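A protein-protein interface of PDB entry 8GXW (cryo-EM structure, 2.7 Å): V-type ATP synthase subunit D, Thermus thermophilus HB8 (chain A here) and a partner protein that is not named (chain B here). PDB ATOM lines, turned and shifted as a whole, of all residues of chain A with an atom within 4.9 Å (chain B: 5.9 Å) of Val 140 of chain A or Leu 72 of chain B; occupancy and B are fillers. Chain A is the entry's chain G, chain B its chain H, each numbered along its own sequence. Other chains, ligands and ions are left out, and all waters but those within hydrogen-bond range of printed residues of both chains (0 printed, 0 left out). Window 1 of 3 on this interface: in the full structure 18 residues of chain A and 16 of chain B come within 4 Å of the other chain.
The guanidinium group of Arg 50 of chain A is in hydrogen-bond range of the side-chain hydroxyl of Tyr 89 of chain B (3.1 Å). OE2 of Glu 144 of chain A is in hydrogen-bond range of OH of Tyr 89 of chain B, at 3.4 Å.
OE1 of Glu 144 of chain A lies within salt-bridge range of NH2 of Arg 50 of chain A, at 3.97 Å. O of Val 45 of chain B is in hydrogen-bond range of N of Leu 72 of chain B, 3.2 Å away. O of Leu 72 of chain B is in hydrogen-bond range of N of Val 47 of chain B (3.4 Å).
Arg 50 of chain A touches Leu 72 of chain B. Val 140 of chain A touches Leu 72 of chain B. CB of Ala 141 of chain A touches CD1 of Leu 44 of chain B, at 3.6 Å. CD1 of Leu 72 of chain B touches CA of Ala 141 of chain A, at 3.9 Å. OE1 of Glu 144 of chain A touches CD1 of Leu 72 of chain B (3.0 Å).
Printed residues of chain B within 4 Å of Arg 50 of chain A: Leu 72 and Tyr 89. Val 140 of chain A touches just one residue of chain B: Leu 72 (3.7 Å). Printed residues of chain A within 4 Å of Leu 44 of chain B: Ala 141. Printed residues of chain A within 4 Å of Tyr 89 of chain B: Arg 50 and Glu 144. The nearest residue of chain A that does not touch Leu 72 of chain B is Leu 137 of chain A (4.5 Å).
Printed residues of chain B that touch a printed residue of chain A: Leu 44, Leu 72 and Tyr 89. Of the 12 printed residues of chain A, 4 touch a printed residue of chain B. Hydrophobic or aromatic side chains of chain A within 4 Å of the printed part of chain B: Val 140 and Ala 141. Among the printed residues, 7 pairs touch across the chains. Among the printed residues, no Asp or Glu carboxylate lies within 4 Å of a Lys or Arg side-chain nitrogen of the other chain.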
ATOM      1  N   ALA A  49       9.809  14.715   3.595  1.00  0.00           N
ATOM      2  CA  ALA A  49       8.512  15.366   3.719  1.00  0.00           C
ATOM      3  C   ALA A  49       8.604  16.603   4.598  1.00  0.00           C
ATOM      4  O   ALA A  49       7.968  17.623   4.314  1.00  0.00           O
ATOM      5  CB  ALA A  49       7.484  14.384   4.280  1.00  0.00           C
ATOM      6  N   ARG A  50       9.386  16.532   5.675  1.00  0.00           N
ATOM      7  CA  ARG A  50       9.501  17.666   6.582  1.00  0.00           C
ATOM      8  C   ARG A  50      10.170  18.854   5.905  1.00  0.00           C
ATOM      9  O   ARG A  50       9.725  19.996   6.067  1.00  0.00           O
ATOM     10  CB  ARG A  50      10.273  17.257   7.834  1.00  0.00           C
ATOM     11  CG  ARG A  50      10.523  18.388   8.817  1.00  0.00           C
ATOM     12  CD  ARG A  50       9.225  19.013   9.295  1.00  0.00           C
ATOM     13  NE  ARG A  50       8.397  18.065  10.031  1.00  0.00           N
ATOM     14  CZ  ARG A  50       8.353  17.966  11.354  1.00  0.00           C
ATOM     15  NH1 ARG A  50       9.095  18.734  12.134  1.00  0.00           N
ATOM     16  NH2 ARG A  50       7.541  17.071  11.909  1.00  0.00           N
ATOM     17  N   LEU A  53       7.735  20.357   3.497  1.00  0.00           N
ATOM     18  CA  LEU A  53       6.736  21.133   4.220  1.00  0.00           C
ATOM     19  C   LEU A  53       7.304  22.466   4.675  1.00  0.00           C
ATOM     20  O   LEU A  53       6.609  23.485   4.649  1.00  0.00           O
ATOM     21  CB  LEU A  53       6.217  20.337   5.416  1.00  0.00           C
ATOM     22  CG  LEU A  53       5.444  21.119   6.481  1.00  0.00           C
ATOM     23  CD1 LEU A  53       4.062  21.475   5.975  1.00  0.00           C
ATOM     24  CD2 LEU A  53       5.358  20.303   7.754  1.00  0.00           C
ATOM     25  N   ALA A 136       0.718  19.600   2.707  1.00  0.00           N
ATOM     26  CA  ALA A 136       2.026  19.246   3.249  1.00  0.00           C
ATOM     27  C   ALA A 136       1.934  18.885   4.726  1.00  0.00           C
ATOM     28  O   ALA A 136       2.602  17.953   5.190  1.00  0.00           O
ATOM     29  CB  ALA A 136       3.006  20.398   3.039  1.00  0.00           C
ATOM     30  N   LEU A 137       1.131  19.631   5.486  1.00  0.00           N
ATOM     31  CA  LEU A 137       0.952  19.322   6.901  1.00  0.00           C
ATOM     32  C   LEU A 137       0.320  17.946   7.076  1.00  0.00           C
ATOM     33  O   LEU A 137       0.734  17.161   7.942  1.00  0.00           O
ATOM     34  CB  LEU A 137       0.093  20.401   7.557  1.00  0.00           C
ATOM     35  CG  LEU A 137      -0.676  20.040   8.831  1.00  0.00           C
ATOM     36  CD1 LEU A 137       0.264  19.559   9.929  1.00  0.00           C
ATOM     37  CD2 LEU A 137      -1.489  21.234   9.309  1.00  0.00           C
ATOM     38  N   ILE A 138      -0.675  17.629   6.251  1.00  0.00           N
ATOM     39  CA  ILE A 138      -1.287  16.306   6.300  1.00  0.00           C
ATOM     40  C   ILE A 138      -0.249  15.237   5.993  1.00  0.00           C
ATOM     41  O   ILE A 138      -0.201  14.192   6.651  1.00  0.00           O
ATOM     42  CB  ILE A 138      -2.478  16.235   5.327  1.00  0.00           C
ATOM     43  CG1 ILE A 138      -3.657  17.048   5.868  1.00  0.00           C
ATOM     44  CG2 ILE A 138      -2.891  14.791   5.103  1.00  0.00           C
ATOM     45  CD1 ILE A 138      -4.687  17.407   4.814  1.00  0.00           C
ATOM     46  N   ARG A 139       0.594  15.476   4.988  1.00  0.00           N
ATOM     47  CA  ARG A 139       1.601  14.482   4.625  1.00  0.00           C
ATOM     48  C   ARG A 139       2.593  14.257   5.760  1.00  0.00           C
ATOM     49  O   ARG A 139       2.947  13.109   6.073  1.00  0.00           O
ATOM     50  CB  ARG A 139       2.331  14.917   3.356  1.00  0.00           C
ATOM     51  CG  ARG A 139       3.101  13.795   2.682  1.00  0.00           C
ATOM     52  CD  ARG A 139       3.412  14.124   1.232  1.00  0.00           C
ATOM     53  NE  ARG A 139       4.276  15.292   1.106  1.00  0.00           N
ATOM     54  CZ  ARG A 139       5.599  15.261   1.189  1.00  0.00           C
ATOM     55  NH1 ARG A 139       6.253  14.130   1.403  1.00  0.00           N
ATOM     56  NH2 ARG A 139       6.284  16.392   1.055  1.00  0.00           N
ATOM     57  N   VAL A 140       3.060  15.338   6.387  1.00  0.00           N
ATOM     58  CA  VAL A 140       4.025  15.188   7.470  1.00  0.00           C
ATOM     59  C   VAL A 140       3.390  14.441   8.632  1.00  0.00           C
ATOM     60  O   VAL A 140       4.021  13.577   9.252  1.00  0.00           O
ATOM     61  CB  VAL A 140       4.593  16.556   7.900  1.00  0.00           C
ATOM     62  CG1 VAL A 140       3.538  17.420   8.548  1.00  0.00           C
ATOM     63  CG2 VAL A 140       5.767  16.370   8.842  1.00  0.00           C
ATOM     64  N   ALA A 141       2.127  14.743   8.938  1.00  0.00           N
ATOM     65  CA  ALA A 141       1.444  14.010   9.996  1.00  0.00           C
ATOM     66  C   ALA A 141       1.331  12.533   9.650  1.00  0.00           C
ATOM     67  O   ALA A 141       1.536  11.664  10.509  1.00  0.00           O
ATOM     68  CB  ALA A 141       0.060  14.610  10.238  1.00  0.00           C
ATOM     69  N   ASN A 142       0.998  12.229   8.395  1.00  0.00           N
ATOM     70  CA  ASN A 142       0.827  10.840   7.992  1.00  0.00           C
ATOM     71  C   ASN A 142       2.121  10.060   8.157  1.00  0.00           C
ATOM     72  O   ASN A 142       2.114   8.929   8.655  1.00  0.00           O
ATOM     73  CB  ASN A 142       0.344  10.770   6.545  1.00  0.00           C
ATOM     74  CG  ASN A 142      -1.115  11.143   6.402  1.00  0.00           C
ATOM     75  OD1 ASN A 142      -1.887  11.057   7.356  1.00  0.00           O
ATOM     76  ND2 ASN A 142      -1.502  11.561   5.203  1.00  0.00           N
ATOM     77  N   THR A 143       3.246  10.644   7.745  1.00  0.00           N
ATOM     78  CA  THR A 143       4.514   9.938   7.918  1.00  0.00           C
ATOM     79  C   THR A 143       4.893   9.836   9.393  1.00  0.00           C
ATOM     80  O   THR A 143       5.418   8.804   9.836  1.00  0.00           O
ATOM     81  CB  THR A 143       5.629  10.615   7.120  1.00  0.00           C
ATOM     82  OG1 THR A 143       6.867   9.934   7.358  1.00  0.00           O
ATOM     83  CG2 THR A 143       5.781  12.073   7.508  1.00  0.00           C
ATOM     84  N   GLU A 144       4.625  10.884  10.175  1.00  0.00           N
ATOM     85  CA  GLU A 144       5.048  10.890  11.571  1.00  0.00           C
ATOM     86  C   GLU A 144       4.304   9.841  12.386  1.00  0.00           C
ATOM     87  O   GLU A 144       4.899   9.171  13.239  1.00  0.00           O
ATOM     88  CB  GLU A 144       4.839  12.280  12.169  1.00  0.00           C
ATOM     89  CG  GLU A 144       5.333  12.421  13.599  1.00  0.00           C
ATOM     90  CD  GLU A 144       5.204  13.835  14.123  1.00  0.00           C
ATOM     91  OE1 GLU A 144       4.709  14.702  13.374  1.00  0.00           O
ATOM     92  OE2 GLU A 144       5.598  14.080  15.283  1.00  0.00           O
ATOM     93  N   LEU B  44      -6.121  16.746  14.712  1.00  0.00           N
ATOM     94  CA  LEU B  44      -4.769  17.284  14.676  1.00  0.00           C
ATOM     95  C   LEU B  44      -4.708  18.623  15.393  1.00  0.00           C
ATOM     96  O   LEU B  44      -5.598  19.464  15.240  1.00  0.00           O
ATOM     97  CB  LEU B  44      -4.274  17.454  13.238  1.00  0.00           C
ATOM     98  CG  LEU B  44      -2.757  17.614  13.125  1.00  0.00           C
ATOM     99  CD1 LEU B  44      -2.220  16.867  11.913  1.00  0.00           C
ATOM    100  CD2 LEU B  44      -2.358  19.082  13.076  1.00  0.00           C
ATOM    101  N   VAL B  45      -3.646  18.812  16.172  1.00  0.00           N
ATOM    102  CA  VAL B  45      -3.360  20.073  16.845  1.00  0.00           C
ATOM    103  C   VAL B  45      -1.895  20.408  16.612  1.00  0.00           C
ATOM    104  O   VAL B  45      -1.017  19.578  16.868  1.00  0.00           O
ATOM    105  CB  VAL B  45      -3.668  20.002  18.353  1.00  0.00           C
ATOM    106  CG1 VAL B  45      -3.405  21.347  19.015  1.00  0.00           C
ATOM    107  CG2 VAL B  45      -5.107  19.560  18.581  1.00  0.00           C
ATOM    108  N   ALA B  46      -1.632  21.619  16.128  1.00  0.00           N
ATOM    109  CA  ALA B  46      -0.275  22.092  15.890  1.00  0.00           C
ATOM    110  C   ALA B  46       0.125  23.047  17.005  1.00  0.00           C
ATOM    111  O   ALA B  46      -0.583  24.024  17.276  1.00  0.00           O
ATOM    112  CB  ALA B  46      -0.166  22.784  14.531  1.00  0.00           C
ATOM    113  N   VAL B  47       1.258  22.766  17.644  1.00  0.00           N
ATOM    114  CA  VAL B  47       1.716  23.511  18.812  1.00  0.00           C
ATOM    115  C   VAL B  47       3.125  24.019  18.543  1.00  0.00           C
ATOM    116  O   VAL B  47       3.986  23.260  18.085  1.00  0.00           O
ATOM    117  CB  VAL B  47       1.692  22.643  20.085  1.00  0.00           C
ATOM    118  CG1 VAL B  47       2.065  23.475  21.302  1.00  0.00           C
ATOM    119  CG2 VAL B  47       0.325  21.996  20.263  1.00  0.00           C
ATOM    120  N   ASP B  48       3.356  25.297  18.827  1.00  0.00           N
ATOM    121  CA  ASP B  48       4.685  25.871  18.672  1.00  0.00           C
ATOM    122  C   ASP B  48       5.614  25.360  19.767  1.00  0.00           C
ATOM    123  O   ASP B  48       5.196  25.147  20.909  1.00  0.00           O
ATOM    124  CB  ASP B  48       4.613  27.397  18.716  1.00  0.00           C
ATOM    125  CG  ASP B  48       4.111  27.996  17.416  1.00  0.00           C
ATOM    126  OD1 ASP B  48       4.370  27.406  16.346  1.00  0.00           O
ATOM    127  OD2 ASP B  48       3.455  29.058  17.464  1.00  0.00           O
ATOM    128  N   PRO B  55       4.109  18.911  23.764  1.00  0.00           N
ATOM    129  CA  PRO B  55       2.719  18.925  24.255  1.00  0.00           C
ATOM    130  C   PRO B  55       2.236  17.565  24.724  1.00  0.00           C
ATOM    131  O   PRO B  55       1.486  17.482  25.706  1.00  0.00           O
ATOM    132  CB  PRO B  55       1.926  19.432  23.042  1.00  0.00           C
ATOM    133  CG  PRO B  55       2.779  19.109  21.863  1.00  0.00           C
ATOM    134  CD  PRO B  55       4.194  19.253  22.334  1.00  0.00           C
ATOM    135  N   VAL B  70      -4.064  14.448  17.130  1.00  0.00           N
ATOM    136  CA  VAL B  70      -2.664  14.304  16.748  1.00  0.00           C
ATOM    137  C   VAL B  70      -1.932  15.586  17.111  1.00  0.00           C
ATOM    138  O   VAL B  70      -2.366  16.681  16.739  1.00  0.00           O
ATOM    139  CB  VAL B  70      -2.515  13.999  15.248  1.00  0.00           C
ATOM    140  CG1 VAL B  70      -1.047  13.981  14.855  1.00  0.00           C
ATOM    141  CG2 VAL B  70      -3.177  12.672  14.908  1.00  0.00           C
ATOM    142  N   LEU B  71      -0.823  15.446  17.830  1.00  0.00           N
ATOM    143  CA  LEU B  71       0.020  16.569  18.220  1.00  0.00           C
ATOM    144  C   LEU B  71       1.280  16.555  17.365  1.00  0.00           C
ATOM    145  O   LEU B  71       1.993  15.548  17.320  1.00  0.00           O
ATOM    146  CB  LEU B  71       0.377  16.498  19.704  1.00  0.00           C
ATOM    147  CG  LEU B  71      -0.786  16.305  20.680  1.00  0.00           C
ATOM    148  CD1 LEU B  71      -0.268  16.250  22.109  1.00  0.00           C
ATOM    149  CD2 LEU B  71      -1.822  17.411  20.525  1.00  0.00           C
ATOM    150  N   LEU B  72       1.549  17.671  16.691  1.00  0.00           N
ATOM    151  CA  LEU B  72       2.735  17.822  15.854  1.00  0.00           C
ATOM    152  C   LEU B  72       3.417  19.130  16.230  1.00  0.00           C
ATOM    153  O   LEU B  72       2.800  20.206  16.092  1.00  0.00           O
ATOM    154  CB  LEU B  72       2.367  17.808  14.370  1.00  0.00           C
ATOM    155  CG  LEU B  72       3.523  17.545  13.402  1.00  0.00           C
ATOM    156  CD1 LEU B  72       3.028  16.826  12.156  1.00  0.00           C
ATOM    157  CD2 LEU B  72       4.226  18.844  13.030  1.00  0.00           C
ATOM    158  N   PRO B  73       4.671  19.107  16.706  1.00  0.00           N
ATOM    159  CA  PRO B  73       5.363  20.375  16.978  1.00  0.00           C
ATOM    160  C   PRO B  73       5.666  21.141  15.701  1.00  0.00           C
ATOM    161  O   PRO B  73       6.492  20.711  14.889  1.00  0.00           O
ATOM    162  CB  PRO B  73       6.649  19.938  17.693  1.00  0.00           C
ATOM    163  CG  PRO B  73       6.425  18.523  18.106  1.00  0.00           C
ATOM    164  CD  PRO B  73       5.475  17.945  17.116  1.00  0.00           C
ATOM    165  N   ILE B  74       5.002  22.275  15.515  1.00  0.00           N
ATOM    166  CA  ILE B  74       5.197  23.118  14.341  1.00  0.00           C
ATOM    167  C   ILE B  74       6.209  24.202  14.677  1.00  0.00           C
ATOM    168  O   ILE B  74       6.238  24.721  15.799  1.00  0.00           O
ATOM    169  CB  ILE B  74       3.861  23.725  13.871  1.00  0.00           C
ATOM    170  CG1 ILE B  74       4.078  24.568  12.613  1.00  0.00           C
ATOM    171  CG2 ILE B  74       3.228  24.567  14.974  1.00  0.00           C
ATOM    172  CD1 ILE B  74       2.803  24.884  11.864  1.00  0.00           C
ATOM    173  N   TYR B  89      15.715  17.839  14.751  1.00  0.00           N
ATOM    174  CA  TYR B  89      14.409  17.349  15.166  1.00  0.00           C
ATOM    175  C   TYR B  89      14.338  15.835  15.037  1.00  0.00           C
ATOM    176  O   TYR B  89      14.013  15.132  16.001  1.00  0.00           O
ATOM    177  CB  TYR B  89      13.312  18.016  14.338  1.00  0.00           C
ATOM    178  CG  TYR B  89      12.056  17.189  14.228  1.00  0.00           C
ATOM    179  CD1 TYR B  89      11.330  16.844  15.359  1.00  0.00           C
ATOM    180  CD2 TYR B  89      11.597  16.749  12.995  1.00  0.00           C
ATOM    181  CE1 TYR B  89      10.185  16.090  15.266  1.00  0.00           C
ATOM    182  CE2 TYR B  89      10.449  15.991  12.892  1.00  0.00           C
ATOM    183  CZ  TYR B  89       9.746  15.664  14.033  1.00  0.00           C
ATOM    184  OH  TYR B  89       8.600  14.909  13.937  1.00  0.00           O
